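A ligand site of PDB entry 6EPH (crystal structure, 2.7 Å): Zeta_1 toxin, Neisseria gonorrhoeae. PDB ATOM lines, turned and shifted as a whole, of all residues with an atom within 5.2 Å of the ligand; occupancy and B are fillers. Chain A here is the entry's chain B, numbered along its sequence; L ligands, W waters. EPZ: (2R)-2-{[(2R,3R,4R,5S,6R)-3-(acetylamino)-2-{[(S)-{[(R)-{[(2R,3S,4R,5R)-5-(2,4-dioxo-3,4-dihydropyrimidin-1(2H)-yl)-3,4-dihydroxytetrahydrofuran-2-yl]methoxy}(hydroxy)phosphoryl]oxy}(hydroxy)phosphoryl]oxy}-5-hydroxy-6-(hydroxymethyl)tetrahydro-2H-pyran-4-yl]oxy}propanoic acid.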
ATOM      1  N   SER A   6      23.797  -9.482 -29.728  1.00  0.00           N
ATOM      2  CA  SER A   6      24.504  -9.263 -28.473  1.00  0.00           C
ATOM      3  C   SER A   6      25.821 -10.042 -28.410  1.00  0.00           C
ATOM      4  O   SER A   6      26.161 -10.767 -29.353  1.00  0.00           O
ATOM      5  CB  SER A   6      23.611  -9.654 -27.295  1.00  0.00           C
ATOM      6  OG  SER A   6      23.215 -11.009 -27.395  1.00  0.00           O
ATOM      7  N   ASP A   7      26.565  -9.855 -27.324  1.00  0.00           N
ATOM      8  CA  ASP A   7      27.769 -10.637 -27.068  1.00  0.00           C
ATOM      9  C   ASP A   7      27.354 -12.002 -26.530  1.00  0.00           C
ATOM     10  O   ASP A   7      26.295 -12.143 -25.918  1.00  0.00           O
ATOM     11  CB  ASP A   7      28.681  -9.921 -26.057  1.00  0.00           C
ATOM     12  CG  ASP A   7      29.212  -8.588 -26.583  1.00  0.00           C
ATOM     13  OD1 ASP A   7      29.483  -8.473 -27.802  1.00  0.00           O
ATOM     14  OD2 ASP A   7      29.375  -7.648 -25.771  1.00  0.00           O
ATOM     15  N   ILE A   8      28.196 -13.017 -26.777  1.00  0.00           N
ATOM     16  CA  ILE A   8      27.915 -14.379 -26.327  1.00  0.00           C
ATOM     17  C   ILE A   8      28.624 -14.610 -24.989  1.00  0.00           C
ATOM     18  O   ILE A   8      29.842 -14.482 -24.909  1.00  0.00           O
ATOM     19  CB  ILE A   8      28.369 -15.422 -27.374  1.00  0.00           C
ATOM     20  CG1 ILE A   8      27.649 -15.162 -28.707  1.00  0.00           C
ATOM     21  CG2 ILE A   8      28.076 -16.837 -26.892  1.00  0.00           C
ATOM     22  CD1 ILE A   8      28.288 -15.818 -29.920  1.00  0.00           C
ATOM     23  N   ASN A   9      27.857 -14.947 -23.958  1.00  0.00           N
ATOM     24  CA  ASN A   9      28.407 -15.146 -22.610  1.00  0.00           C
ATOM     25  C   ASN A   9      29.197 -16.447 -22.531  1.00  0.00           C
ATOM     26  O   ASN A   9      28.673 -17.504 -22.880  1.00  0.00           O
ATOM     27  CB  ASN A   9      27.295 -15.190 -21.553  1.00  0.00           C
ATOM     28  CG  ASN A   9      26.512 -13.886 -21.446  1.00  0.00           C
ATOM     29  OD1 ASN A   9      27.045 -12.797 -21.694  1.00  0.00           O
ATOM     30  ND2 ASN A   9      25.236 -13.995 -21.081  1.00  0.00           N
ATOM     31  N   ARG A  11      30.961 -19.513 -20.539  1.00  0.00           N
ATOM     32  CA  ARG A  11      30.884 -20.295 -19.308  1.00  0.00           C
ATOM     33  C   ARG A  11      32.284 -20.729 -18.906  1.00  0.00           C
ATOM     34  O   ARG A  11      33.186 -20.797 -19.743  1.00  0.00           O
ATOM     35  CB  ARG A  11      29.982 -21.509 -19.506  1.00  0.00           C
ATOM     36  CG  ARG A  11      28.663 -21.183 -20.171  1.00  0.00           C
ATOM     37  CD  ARG A  11      27.621 -22.230 -19.836  1.00  0.00           C
ATOM     38  NE  ARG A  11      26.393 -22.057 -20.598  1.00  0.00           N
ATOM     39  CZ  ARG A  11      25.244 -22.676 -20.337  1.00  0.00           C
ATOM     40  NH1 ARG A  11      25.120 -23.518 -19.306  1.00  0.00           N
ATOM     41  NH2 ARG A  11      24.183 -22.444 -21.115  1.00  0.00           N
ATOM     42  N   CYS A  54      14.261 -20.631 -32.591  1.00  0.00           N
ATOM     43  CA  CYS A  54      14.563 -21.447 -31.415  1.00  0.00           C
ATOM     44  C   CYS A  54      16.053 -21.755 -31.334  1.00  0.00           C
ATOM     45  O   CYS A  54      16.665 -22.141 -32.340  1.00  0.00           O
ATOM     46  CB  CYS A  54      13.768 -22.741 -31.474  1.00  0.00           C
ATOM     47  SG  CYS A  54      13.956 -23.763 -30.004  1.00  0.00           S
ATOM     48  N   ALA A  55      16.622 -21.614 -30.142  1.00  0.00           N
ATOM     49  CA  ALA A  55      18.039 -21.910 -29.924  1.00  0.00           C
ATOM     50  C   ALA A  55      18.366 -23.399 -30.150  1.00  0.00           C
ATOM     51  O   ALA A  55      19.451 -23.716 -30.641  1.00  0.00           O
ATOM     52  CB  ALA A  55      18.465 -21.479 -28.532  1.00  0.00           C
ATOM     53  N   ASP A  56      17.448 -24.299 -29.808  1.00  0.00           N
ATOM     54  CA  ASP A  56      17.660 -25.750 -30.017  1.00  0.00           C
ATOM     55  C   ASP A  56      17.804 -26.124 -31.488  1.00  0.00           C
ATOM     56  O   ASP A  56      18.654 -26.933 -31.830  1.00  0.00           O
ATOM     57  CB  ASP A  56      16.516 -26.568 -29.417  1.00  0.00           C
ATOM     58  CG  ASP A  56      16.710 -26.823 -27.948  1.00  0.00           C
ATOM     59  OD1 ASP A  56      17.668 -27.546 -27.599  1.00  0.00           O
ATOM     60  OD2 ASP A  56      15.906 -26.306 -27.139  1.00  0.00           O
ATOM     61  N   LYS A  59      21.249 -25.189 -32.814  1.00  0.00           N
ATOM     62  CA  LYS A  59      22.325 -26.108 -32.449  1.00  0.00           C
ATOM     63  C   LYS A  59      22.677 -27.081 -33.571  1.00  0.00           C
ATOM     64  O   LYS A  59      23.852 -27.418 -33.741  1.00  0.00           O
ATOM     65  CB  LYS A  59      21.976 -26.896 -31.184  1.00  0.00           C
ATOM     66  CG  LYS A  59      21.952 -26.067 -29.918  1.00  0.00           C
ATOM     67  CD  LYS A  59      21.345 -26.851 -28.773  1.00  0.00           C
ATOM     68  CE  LYS A  59      21.151 -25.984 -27.553  1.00  0.00           C
ATOM     69  NZ  LYS A  59      20.311 -26.704 -26.563  1.00  0.00           N
ATOM     70  N   ASN A  75      26.477 -29.652 -25.579  1.00  0.00           N
ATOM     71  CA  ASN A  75      25.302 -28.777 -25.491  1.00  0.00           C
ATOM     72  C   ASN A  75      25.539 -27.441 -24.773  1.00  0.00           C
ATOM     73  O   ASN A  75      25.274 -26.378 -25.338  1.00  0.00           O
ATOM     74  CB  ASN A  75      24.151 -29.508 -24.780  1.00  0.00           C
ATOM     75  CG  ASN A  75      22.863 -28.733 -24.812  1.00  0.00           C
ATOM     76  OD1 ASN A  75      22.384 -28.357 -25.879  1.00  0.00           O
ATOM     77  ND2 ASN A  75      22.292 -28.502 -23.641  1.00  0.00           N
ATOM     78  N   ASN A  76      26.045 -27.505 -23.548  1.00  0.00           N
ATOM     79  CA  ASN A  76      26.278 -26.309 -22.729  1.00  0.00           C
ATOM     80  C   ASN A  76      27.422 -25.436 -23.266  1.00  0.00           C
ATOM     81  O   ASN A  76      27.503 -24.250 -22.926  1.00  0.00           O
ATOM     82  CB  ASN A  76      26.546 -26.686 -21.264  1.00  0.00           C
ATOM     83  CG  ASN A  76      25.350 -27.334 -20.572  1.00  0.00           C
ATOM     84  OD1 ASN A  76      24.254 -27.447 -21.141  1.00  0.00           O
ATOM     85  ND2 ASN A  76      25.550 -27.765 -19.331  1.00  0.00           N
ATOM     86  N   HIS A  79      25.359 -23.712 -26.520  1.00  0.00           N
ATOM     87  CA  HIS A  79      24.016 -23.146 -26.297  1.00  0.00           C
ATOM     88  C   HIS A  79      23.900 -21.621 -26.415  1.00  0.00           C
ATOM     89  O   HIS A  79      22.990 -21.115 -27.097  1.00  0.00           O
ATOM     90  CB  HIS A  79      23.462 -23.565 -24.930  1.00  0.00           C
ATOM     91  CG  HIS A  79      22.156 -22.927 -24.598  1.00  0.00           C
ATOM     92  ND1 HIS A  79      20.953 -23.394 -25.077  1.00  0.00           N
ATOM     93  CD2 HIS A  79      21.863 -21.817 -23.875  1.00  0.00           C
ATOM     94  CE1 HIS A  79      19.975 -22.619 -24.644  1.00  0.00           C
ATOM     95  NE2 HIS A  79      20.506 -21.659 -23.909  1.00  0.00           N
ATOM     96  N   ASN A  80      24.783 -20.903 -25.731  1.00  0.00           N
ATOM     97  CA  ASN A  80      24.761 -19.437 -25.734  1.00  0.00           C
ATOM     98  C   ASN A  80      24.989 -18.860 -27.136  1.00  0.00           C
ATOM     99  O   ASN A  80      24.391 -17.839 -27.480  1.00  0.00           O
ATOM    100  CB  ASN A  80      25.795 -18.853 -24.751  1.00  0.00           C
ATOM    101  CG  ASN A  80      25.398 -19.049 -23.294  1.00  0.00           C
ATOM    102  OD1 ASN A  80      24.388 -19.688 -22.973  1.00  0.00           O
ATOM    103  ND2 ASN A  80      26.204 -18.499 -22.390  1.00  0.00           N
ATOM    104  N   ALA A  83      21.683 -19.487 -28.806  1.00  0.00           N
ATOM    105  CA  ALA A  83      20.669 -18.587 -28.238  1.00  0.00           C
ATOM    106  C   ALA A  83      20.816 -17.156 -28.772  1.00  0.00           C
ATOM    107  O   ALA A  83      19.812 -16.512 -29.084  1.00  0.00           O
ATOM    108  CB  ALA A  83      20.745 -18.603 -26.716  1.00  0.00           C
ATOM    109  N   VAL A  84      22.046 -16.674 -28.874  1.00  0.00           N
ATOM    110  CA  VAL A  84      22.326 -15.347 -29.442  1.00  0.00           C
ATOM    111  C   VAL A  84      22.043 -15.330 -30.949  1.00  0.00           C
ATOM    112  O   VAL A  84      21.594 -14.315 -31.480  1.00  0.00           O
ATOM    113  CB  VAL A  84      23.768 -14.874 -29.134  1.00  0.00           C
ATOM    114  CG1 VAL A  84      24.127 -13.584 -29.872  1.00  0.00           C
ATOM    115  CG2 VAL A  84      23.943 -14.673 -27.629  1.00  0.00           C
ATOM    116  N   SER A  86      19.658 -17.181 -32.302  1.00  0.00           N
ATOM    117  CA  SER A  86      18.193 -17.154 -32.337  1.00  0.00           C
ATOM    118  C   SER A  86      17.669 -15.745 -32.048  1.00  0.00           C
ATOM    119  O   SER A  86      16.733 -15.291 -32.681  1.00  0.00           O
ATOM    120  CB  SER A  86      17.594 -18.169 -31.356  1.00  0.00           C
ATOM    121  OG  SER A  86      17.768 -17.764 -30.016  1.00  0.00           O
ATOM    122  N   SER A  87      18.301 -15.066 -31.101  1.00  0.00           N
ATOM    123  CA  SER A  87      17.985 -13.671 -30.807  1.00  0.00           C
ATOM    124  C   SER A  87      18.244 -12.758 -31.999  1.00  0.00           C
ATOM    125  O   SER A  87      17.462 -11.846 -32.272  1.00  0.00           O
ATOM    126  CB  SER A  87      18.803 -13.189 -29.616  1.00  0.00           C
ATOM    127  OG  SER A  87      18.473 -11.853 -29.268  1.00  0.00           O
ATOM    128  N   GLY A 109       8.068 -23.256 -21.503  1.00  0.00           N
ATOM    129  CA  GLY A 109       7.781 -24.413 -20.670  1.00  0.00           C
ATOM    130  C   GLY A 109       8.993 -25.296 -20.441  1.00  0.00           C
ATOM    131  O   GLY A 109      10.005 -25.214 -21.137  1.00  0.00           O
ATOM    132  N   PRO A 111      11.568 -28.394 -20.400  1.00  0.00           N
ATOM    133  CA  PRO A 111      11.962 -29.392 -21.403  1.00  0.00           C
ATOM    134  C   PRO A 111      11.221 -30.725 -21.237  1.00  0.00           C
ATOM    135  O   PRO A 111      11.084 -31.218 -20.109  1.00  0.00           O
ATOM    136  CB  PRO A 111      13.459 -29.588 -21.138  1.00  0.00           C
ATOM    137  CG  PRO A 111      13.900 -28.279 -20.604  1.00  0.00           C
ATOM    138  CD  PRO A 111      12.751 -27.776 -19.764  1.00  0.00           C
ATOM    139  N   LYS A 115       6.551 -28.697 -26.188  1.00  0.00           N
ATOM    140  CA  LYS A 115       6.523 -27.354 -26.751  1.00  0.00           C
ATOM    141  C   LYS A 115       6.662 -27.417 -28.254  1.00  0.00           C
ATOM    142  O   LYS A 115       5.822 -26.874 -28.988  1.00  0.00           O
ATOM    143  CB  LYS A 115       7.669 -26.508 -26.194  1.00  0.00           C
ATOM    144  CG  LYS A 115       7.562 -26.186 -24.720  1.00  0.00           C
ATOM    145  CD  LYS A 115       8.549 -25.098 -24.290  1.00  0.00           C
ATOM    146  CE  LYS A 115      10.011 -25.433 -24.560  1.00  0.00           C
ATOM    147  NZ  LYS A 115      10.488 -26.634 -23.838  1.00  0.00           N
ATOM    148  N   PHE A 132       8.544 -17.724 -31.362  1.00  0.00           N
ATOM    149  CA  PHE A 132       9.792 -17.910 -30.605  1.00  0.00           C
ATOM    150  C   PHE A 132       9.608 -18.925 -29.473  1.00  0.00           C
ATOM    151  O   PHE A 132       8.775 -18.737 -28.599  1.00  0.00           O
ATOM    152  CB  PHE A 132      10.283 -16.578 -30.027  1.00  0.00           C
ATOM    153  CG  PHE A 132      11.563 -16.688 -29.253  1.00  0.00           C
ATOM    154  CD1 PHE A 132      12.794 -16.765 -29.911  1.00  0.00           C
ATOM    155  CD2 PHE A 132      11.547 -16.764 -27.858  1.00  0.00           C
ATOM    156  CE1 PHE A 132      13.973 -16.894 -29.200  1.00  0.00           C
ATOM    157  CE2 PHE A 132      12.737 -16.900 -27.143  1.00  0.00           C
ATOM    158  CZ  PHE A 132      13.950 -16.959 -27.818  1.00  0.00           C
ATOM    159  N   GLU A 133      10.401 -19.997 -29.507  1.00  0.00           N
ATOM    160  CA  GLU A 133      10.416 -20.995 -28.451  1.00  0.00           C
ATOM    161  C   GLU A 133      11.642 -20.771 -27.590  1.00  0.00           C
ATOM    162  O   GLU A 133      12.756 -20.690 -28.103  1.00  0.00           O
ATOM    163  CB  GLU A 133      10.424 -22.395 -29.045  1.00  0.00           C
ATOM    164  CG  GLU A 133      10.137 -23.497 -28.034  1.00  0.00           C
ATOM    165  CD  GLU A 133      10.201 -24.884 -28.636  1.00  0.00           C
ATOM    166  OE1 GLU A 133      10.812 -25.783 -28.021  1.00  0.00           O
ATOM    167  OE2 GLU A 133       9.639 -25.071 -29.740  1.00  0.00           O
ATOM    168  N   GLY A 134      11.428 -20.682 -26.280  1.00  0.00           N
ATOM    169  CA  GLY A 134      12.507 -20.357 -25.332  1.00  0.00           C
ATOM    170  C   GLY A 134      11.990 -20.125 -23.918  1.00  0.00           C
ATOM    171  O   GLY A 134      10.788 -19.948 -23.710  1.00  0.00           O
ATOM    172  N   GLN A 135      12.909 -20.130 -22.954  1.00  0.00           N
ATOM    173  CA  GLN A 135      12.533 -19.959 -21.550  1.00  0.00           C
ATOM    174  C   GLN A 135      12.150 -18.516 -21.253  1.00  0.00           C
ATOM    175  O   GLN A 135      12.787 -17.583 -21.745  1.00  0.00           O
ATOM    176  CB  GLN A 135      13.654 -20.425 -20.605  1.00  0.00           C
ATOM    177  CG  GLN A 135      14.892 -19.532 -20.542  1.00  0.00           C
ATOM    178  CD  GLN A 135      14.787 -18.355 -19.586  1.00  0.00           C
ATOM    179  OE1 GLN A 135      13.908 -18.314 -18.720  1.00  0.00           O
ATOM    180  NE2 GLN A 135      15.686 -17.407 -19.740  1.00  0.00           N
ATOM    181  N   SER A 141      15.814 -11.111 -20.777  1.00  0.00           N
ATOM    182  CA  SER A 141      16.054 -11.136 -22.207  1.00  0.00           C
ATOM    183  C   SER A 141      14.772 -11.059 -23.049  1.00  0.00           C
ATOM    184  O   SER A 141      14.774 -10.474 -24.136  1.00  0.00           O
ATOM    185  CB  SER A 141      16.821 -12.398 -22.589  1.00  0.00           C
ATOM    186  OG  SER A 141      17.220 -12.297 -23.933  1.00  0.00           O
ATOM    187  N   ARG A 144      13.351  -7.422 -23.757  1.00  0.00           N
ATOM    188  CA  ARG A 144      13.854  -6.738 -24.951  1.00  0.00           C
ATOM    189  C   ARG A 144      13.126  -7.216 -26.208  1.00  0.00           C
ATOM    190  O   ARG A 144      12.857  -6.405 -27.094  1.00  0.00           O
ATOM    191  CB  ARG A 144      15.366  -6.946 -25.145  1.00  0.00           C
ATOM    192  CG  ARG A 144      16.264  -6.500 -23.994  1.00  0.00           C
ATOM    193  CD  ARG A 144      17.728  -6.387 -24.449  1.00  0.00           C
ATOM    194  NE  ARG A 144      18.690  -7.060 -23.562  1.00  0.00           N
ATOM    195  CZ  ARG A 144      18.927  -8.382 -23.517  1.00  0.00           C
ATOM    196  NH1 ARG A 144      18.276  -9.240 -24.300  1.00  0.00           N
ATOM    197  NH2 ARG A 144      19.832  -8.863 -22.673  1.00  0.00           N
ATOM    198  N   LYS A 145      12.798  -8.504 -26.283  1.00  0.00           N
ATOM    199  CA  LYS A 145      12.077  -9.075 -27.435  1.00  0.00           C
ATOM    200  C   LYS A 145      10.643  -8.562 -27.491  1.00  0.00           C
ATOM    201  O   LYS A 145      10.179  -8.128 -28.548  1.00  0.00           O
ATOM    202  CB  LYS A 145      12.062 -10.606 -27.397  1.00  0.00           C
ATOM    203  CG  LYS A 145      13.433 -11.244 -27.581  1.00  0.00           C
ATOM    204  CD  LYS A 145      13.342 -12.744 -27.836  1.00  0.00           C
ATOM    205  CE  LYS A 145      14.728 -13.357 -28.000  1.00  0.00           C
ATOM    206  NZ  LYS A 145      15.560 -13.292 -26.768  1.00  0.00           N
ATOM    207  N   GLY A 182      18.757 -34.817 -24.547  1.00  0.00           N
ATOM    208  CA  GLY A 182      17.943 -34.822 -23.336  1.00  0.00           C
ATOM    209  C   GLY A 182      17.974 -33.446 -22.701  1.00  0.00           C
ATOM    210  O   GLY A 182      18.262 -32.452 -23.348  1.00  0.00           O
ATOM    211  N   ALA A 183      17.652 -33.419 -21.414  1.00  0.00           N
ATOM    212  CA  ALA A 183      17.654 -32.201 -20.624  1.00  0.00           C
ATOM    213  C   ALA A 183      18.141 -32.531 -19.236  1.00  0.00           C
ATOM    214  O   ALA A 183      17.842 -33.615 -18.726  1.00  0.00           O
ATOM    215  CB  ALA A 183      16.249 -31.631 -20.570  1.00  0.00           C
ATOM    216  N   ILE A 187      18.247 -27.638 -14.922  1.00  0.00           N
ATOM    217  CA  ILE A 187      17.542 -26.682 -15.767  1.00  0.00           C
ATOM    218  C   ILE A 187      16.031 -26.946 -15.810  1.00  0.00           C
ATOM    219  O   ILE A 187      15.243 -26.002 -15.905  1.00  0.00           O
ATOM    220  CB  ILE A 187      18.164 -26.633 -17.178  1.00  0.00           C
ATOM    221  CG1 ILE A 187      17.751 -25.341 -17.895  1.00  0.00           C
ATOM    222  CG2 ILE A 187      17.781 -27.851 -18.031  1.00  0.00           C
ATOM    223  CD1 ILE A 187      18.631 -25.030 -19.078  1.00  0.00           C
ATOM    224  N   ILE A 191      13.586 -23.935 -14.620  1.00  0.00           N
ATOM    225  CA  ILE A 191      12.520 -23.407 -15.475  1.00  0.00           C
ATOM    226  C   ILE A 191      11.149 -23.584 -14.819  1.00  0.00           C
ATOM    227  O   ILE A 191      10.416 -22.604 -14.682  1.00  0.00           O
ATOM    228  CB  ILE A 191      12.572 -24.023 -16.897  1.00  0.00           C
ATOM    229  CG1 ILE A 191      13.786 -23.468 -17.645  1.00  0.00           C
ATOM    230  CG2 ILE A 191      11.295 -23.723 -17.688  1.00  0.00           C
ATOM    231  CD1 ILE A 191      14.120 -24.164 -18.952  1.00  0.00           C
HETATM  232  C1  EPZ L   1      16.212 -22.102 -22.665  1.00  0.00           C
HETATM  233  O1  EPZ L   1      16.894 -21.721 -23.835  1.00  0.00           O
HETATM  234  C2  EPZ L   1      17.018 -23.211 -21.962  1.00  0.00           C
HETATM  235  N2  EPZ L   1      18.376 -22.815 -21.655  1.00  0.00           N
HETATM  236  C3  EPZ L   1      16.974 -24.478 -22.814  1.00  0.00           C
HETATM  237  O3  EPZ L   1      17.590 -25.549 -22.081  1.00  0.00           O
HETATM  238  C4  EPZ L   1      15.539 -24.881 -23.138  1.00  0.00           C
HETATM  239  O4  EPZ L   1      15.529 -25.999 -24.017  1.00  0.00           O
HETATM  240  C5  EPZ L   1      14.802 -23.720 -23.797  1.00  0.00           C
HETATM  241  O5  EPZ L   1      14.893 -22.537 -22.976  1.00  0.00           O
HETATM  242  C6  EPZ L   1      13.302 -23.978 -23.971  1.00  0.00           C
HETATM  243  O6  EPZ L   1      12.988 -24.363 -25.305  1.00  0.00           O
HETATM  244  C7  EPZ L   1      18.838 -22.000 -20.684  1.00  0.00           C
HETATM  245  O7  EPZ L   1      19.995 -21.602 -20.666  1.00  0.00           O
HETATM  246  C8  EPZ L   1      17.863 -21.611 -19.599  1.00  0.00           C
HETATM  247  PA  EPZ L   1      18.733 -18.642 -22.829  1.00  0.00           P
HETATM  248  PB  EPZ L   1      16.917 -20.273 -24.382  1.00  0.00           P
HETATM  249  O1A EPZ L   1      20.073 -19.058 -22.293  1.00  0.00           O
HETATM  250  O1B EPZ L   1      16.928 -20.358 -25.930  1.00  0.00           O
HETATM  251  C1D EPZ L   1      19.807 -13.847 -24.657  1.00  0.00           C
HETATM  252  C1E EPZ L   1      19.881 -25.985 -22.854  1.00  0.00           C
HETATM  253  O1E EPZ L   1      20.163 -25.038 -21.998  1.00  0.00           O
HETATM  254  N1U EPZ L   1      21.197 -14.337 -24.455  1.00  0.00           N
HETATM  255  O2A EPZ L   1      17.670 -18.634 -21.703  1.00  0.00           O
HETATM  256  O2B EPZ L   1      15.727 -19.488 -23.932  1.00  0.00           O
HETATM  257  C2D EPZ L   1      19.251 -14.053 -26.075  1.00  0.00           C
HETATM  258  O2D EPZ L   1      18.411 -12.981 -26.458  1.00  0.00           O
HETATM  259  C2E EPZ L   1      18.441 -26.437 -22.843  1.00  0.00           C
HETATM  260  O2E EPZ L   1      20.690 -26.465 -23.617  1.00  0.00           O
HETATM  261  C2U EPZ L   1      22.239 -13.403 -24.455  1.00  0.00           C
HETATM  262  O2U EPZ L   1      22.048 -12.206 -24.615  1.00  0.00           O
HETATM  263  O3A EPZ L   1      18.246 -19.605 -23.947  1.00  0.00           O
HETATM  264  C3D EPZ L   1      18.517 -15.390 -25.933  1.00  0.00           C
HETATM  265  O3D EPZ L   1      17.474 -15.512 -26.895  1.00  0.00           O
HETATM  266  C3E EPZ L   1      18.349 -27.827 -22.227  1.00  0.00           C
HETATM  267  N3U EPZ L   1      23.495 -13.925 -24.254  1.00  0.00           N
HETATM  268  C4D EPZ L   1      17.938 -15.255 -24.539  1.00  0.00           C
HETATM  269  O4D EPZ L   1      18.960 -14.570 -23.789  1.00  0.00           O
HETATM  270  C4U EPZ L   1      23.825 -15.257 -24.060  1.00  0.00           C
HETATM  271  O4U EPZ L   1      25.034 -15.572 -23.901  1.00  0.00           O
HETATM  272  C5D EPZ L   1      17.588 -16.545 -23.846  1.00  0.00           C
HETATM  273  O5D EPZ L   1      18.793 -17.238 -23.474  1.00  0.00           O
HETATM  274  C5U EPZ L   1      22.721 -16.159 -24.075  1.00  0.00           C
HETATM  275  C6U EPZ L   1      21.466 -15.671 -24.265  1.00  0.00           C
HETATM  276  O   HOH W   1      16.373 -10.791 -26.132  1.00  0.00           O
HETATM  277  O   HOH W   2      11.202 -22.889 -21.800  1.00  0.00           O
HETATM  278  O   HOH W   3      17.086 -20.368 -16.880  1.00  0.00           O
HETATM  279  O   HOH W   4      17.346 -18.114 -27.178  1.00  0.00           O
HETATM  280  O   HOH W   5      13.298 -27.762 -24.146  1.00  0.00           O
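The side-chain amide nitrogen (ND2) of Asn 80 sits at hydrogen-bond distance from the backbone carbonyl oxygen (O) of Asn 9. OG of Ser 141 sits at hydrogen-bond distance from NZ of Lys 145, 3.4 Å away. NZ of Lys 59 lies within salt-bridge range of OD1 of Asp 56 (3.0 Å). N of Asp 56 lies close to SG of Cys 54 (3.5 Å). The guanidinium group of Arg 144 is in hydrogen-bond range of the side-chain hydroxyl of Ser 141. NZ of Lys 59 lies within hydrogen-bond range of OD1 of Asn 75. The side-chain hydroxyl of Ser 86 is in hydrogen-bond range of the backbone carbonyl oxygen of Ala 83, at 2.6 Å. ND2 of Asn 75 lies within hydrogen-bond range of OD1 of Asn 76.
Water W4 lies within hydrogen-bond range of O1B of the ligand (2.6 Å) and OG of Ser 86 (2.9 Å). Water W5 bridges O4 of the ligand and NZ of Lys 115. Water W1 lies within hydrogen-bond range of the backbone carbonyl oxygen (O) of Ser 141, the side-chain amino group (NZ) of Lys 145, an oxygen (O2D) of the ligand and the guanidinium group (NH1) of Arg 144. Water W2 bridges O of Gly 109 (2.7 Å) and N of Gln 135 (3.4 Å).
O of Asp 7 touches N3U of the ligand (3.7 Å). Ile 8 touches the ligand (C to O4U, 3.9 Å). Ala 55 touches the ligand. Val 84 touches the ligand (CG2 to N3U, 3.5 Å). Ser 86 touches the ligand. Lys 115 touches the ligand. CZ of Phe 132 touches O3D of the ligand, at 3.9 Å. Glu 133 touches the ligand. Gly 134 touches the ligand. CD1 of Ile 187 touches O3 of the ligand, 3.2 Å away. Hydrophobic or aromatic side chains that line the ligand: Ala 55, His 79, Ala 83, Val 84, Phe 132 and Ile 187. 22 residues have an atom within 4 Å of the ligand: Ser 6, Asp 7, Ile 8, Asn 9, Ala 55, Asp 56, Lys 59, Asn 75, His 79, Asn 80, Ala 83, Val 84, Ser 86, Ser 87, Lys 115, Phe 132, Glu 133, Gly 134, Gln 135, Ser 141, Lys 145 and Ile 187.
The side-chain amino group (NZ) of Lys 59 is in salt-bridge range of an oxygen (O2E) of the ligand (3.0 Å). An oxygen (O2B) of the ligand is in hydrogen-bond range of the backbone NH (N) of Gln 135. An oxygen (O2D) of the ligand lies within hydrogen-bond range of the side-chain amino group of Lys 145, at 2.9 Å. An oxygen (O3D) of the ligand is in hydrogen-bond range of the backbone carbonyl oxygen (O) of Ala 83 (3.4 Å). O4U of the ligand sits close to ND2 of Asn 80. OD2 of Asp 56 sits at hydrogen-bond distance from O4 of the ligand (3.2 Å). The side-chain amide nitrogen (NE2) of Gln 135 lies within hydrogen-bond range of an oxygen (O2A) of the ligand. OG of Ser 87 lies within hydrogen-bond range of O2D of the ligand (3.0 Å). The side-chain amide nitrogen of Asn 9 lies within hydrogen-bond range of an oxygen (O4U) of the ligand, at 3.2 Å. An oxygen (O3A) of the ligand sits at hydrogen-bond distance from a ring nitrogen (NE2) of His 79. The side-chain hydroxyl (OG) of Ser 141 lies within hydrogen-bond range of an oxygen (O4D) of the ligand, 2.9 Å away. OG of Ser 6 sits at hydrogen-bond distance from O2U of the ligand (3.2 Å). An oxygen (O4U) of the ligand sits at hydrogen-bond distance from the backbone NH (N) of Asn 9 (2.9 Å). The side-chain amide nitrogen (ND2) of Asn 75 lies within hydrogen-bond range of an oxygen (O2E) of the ligand, at 2.6 Å.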
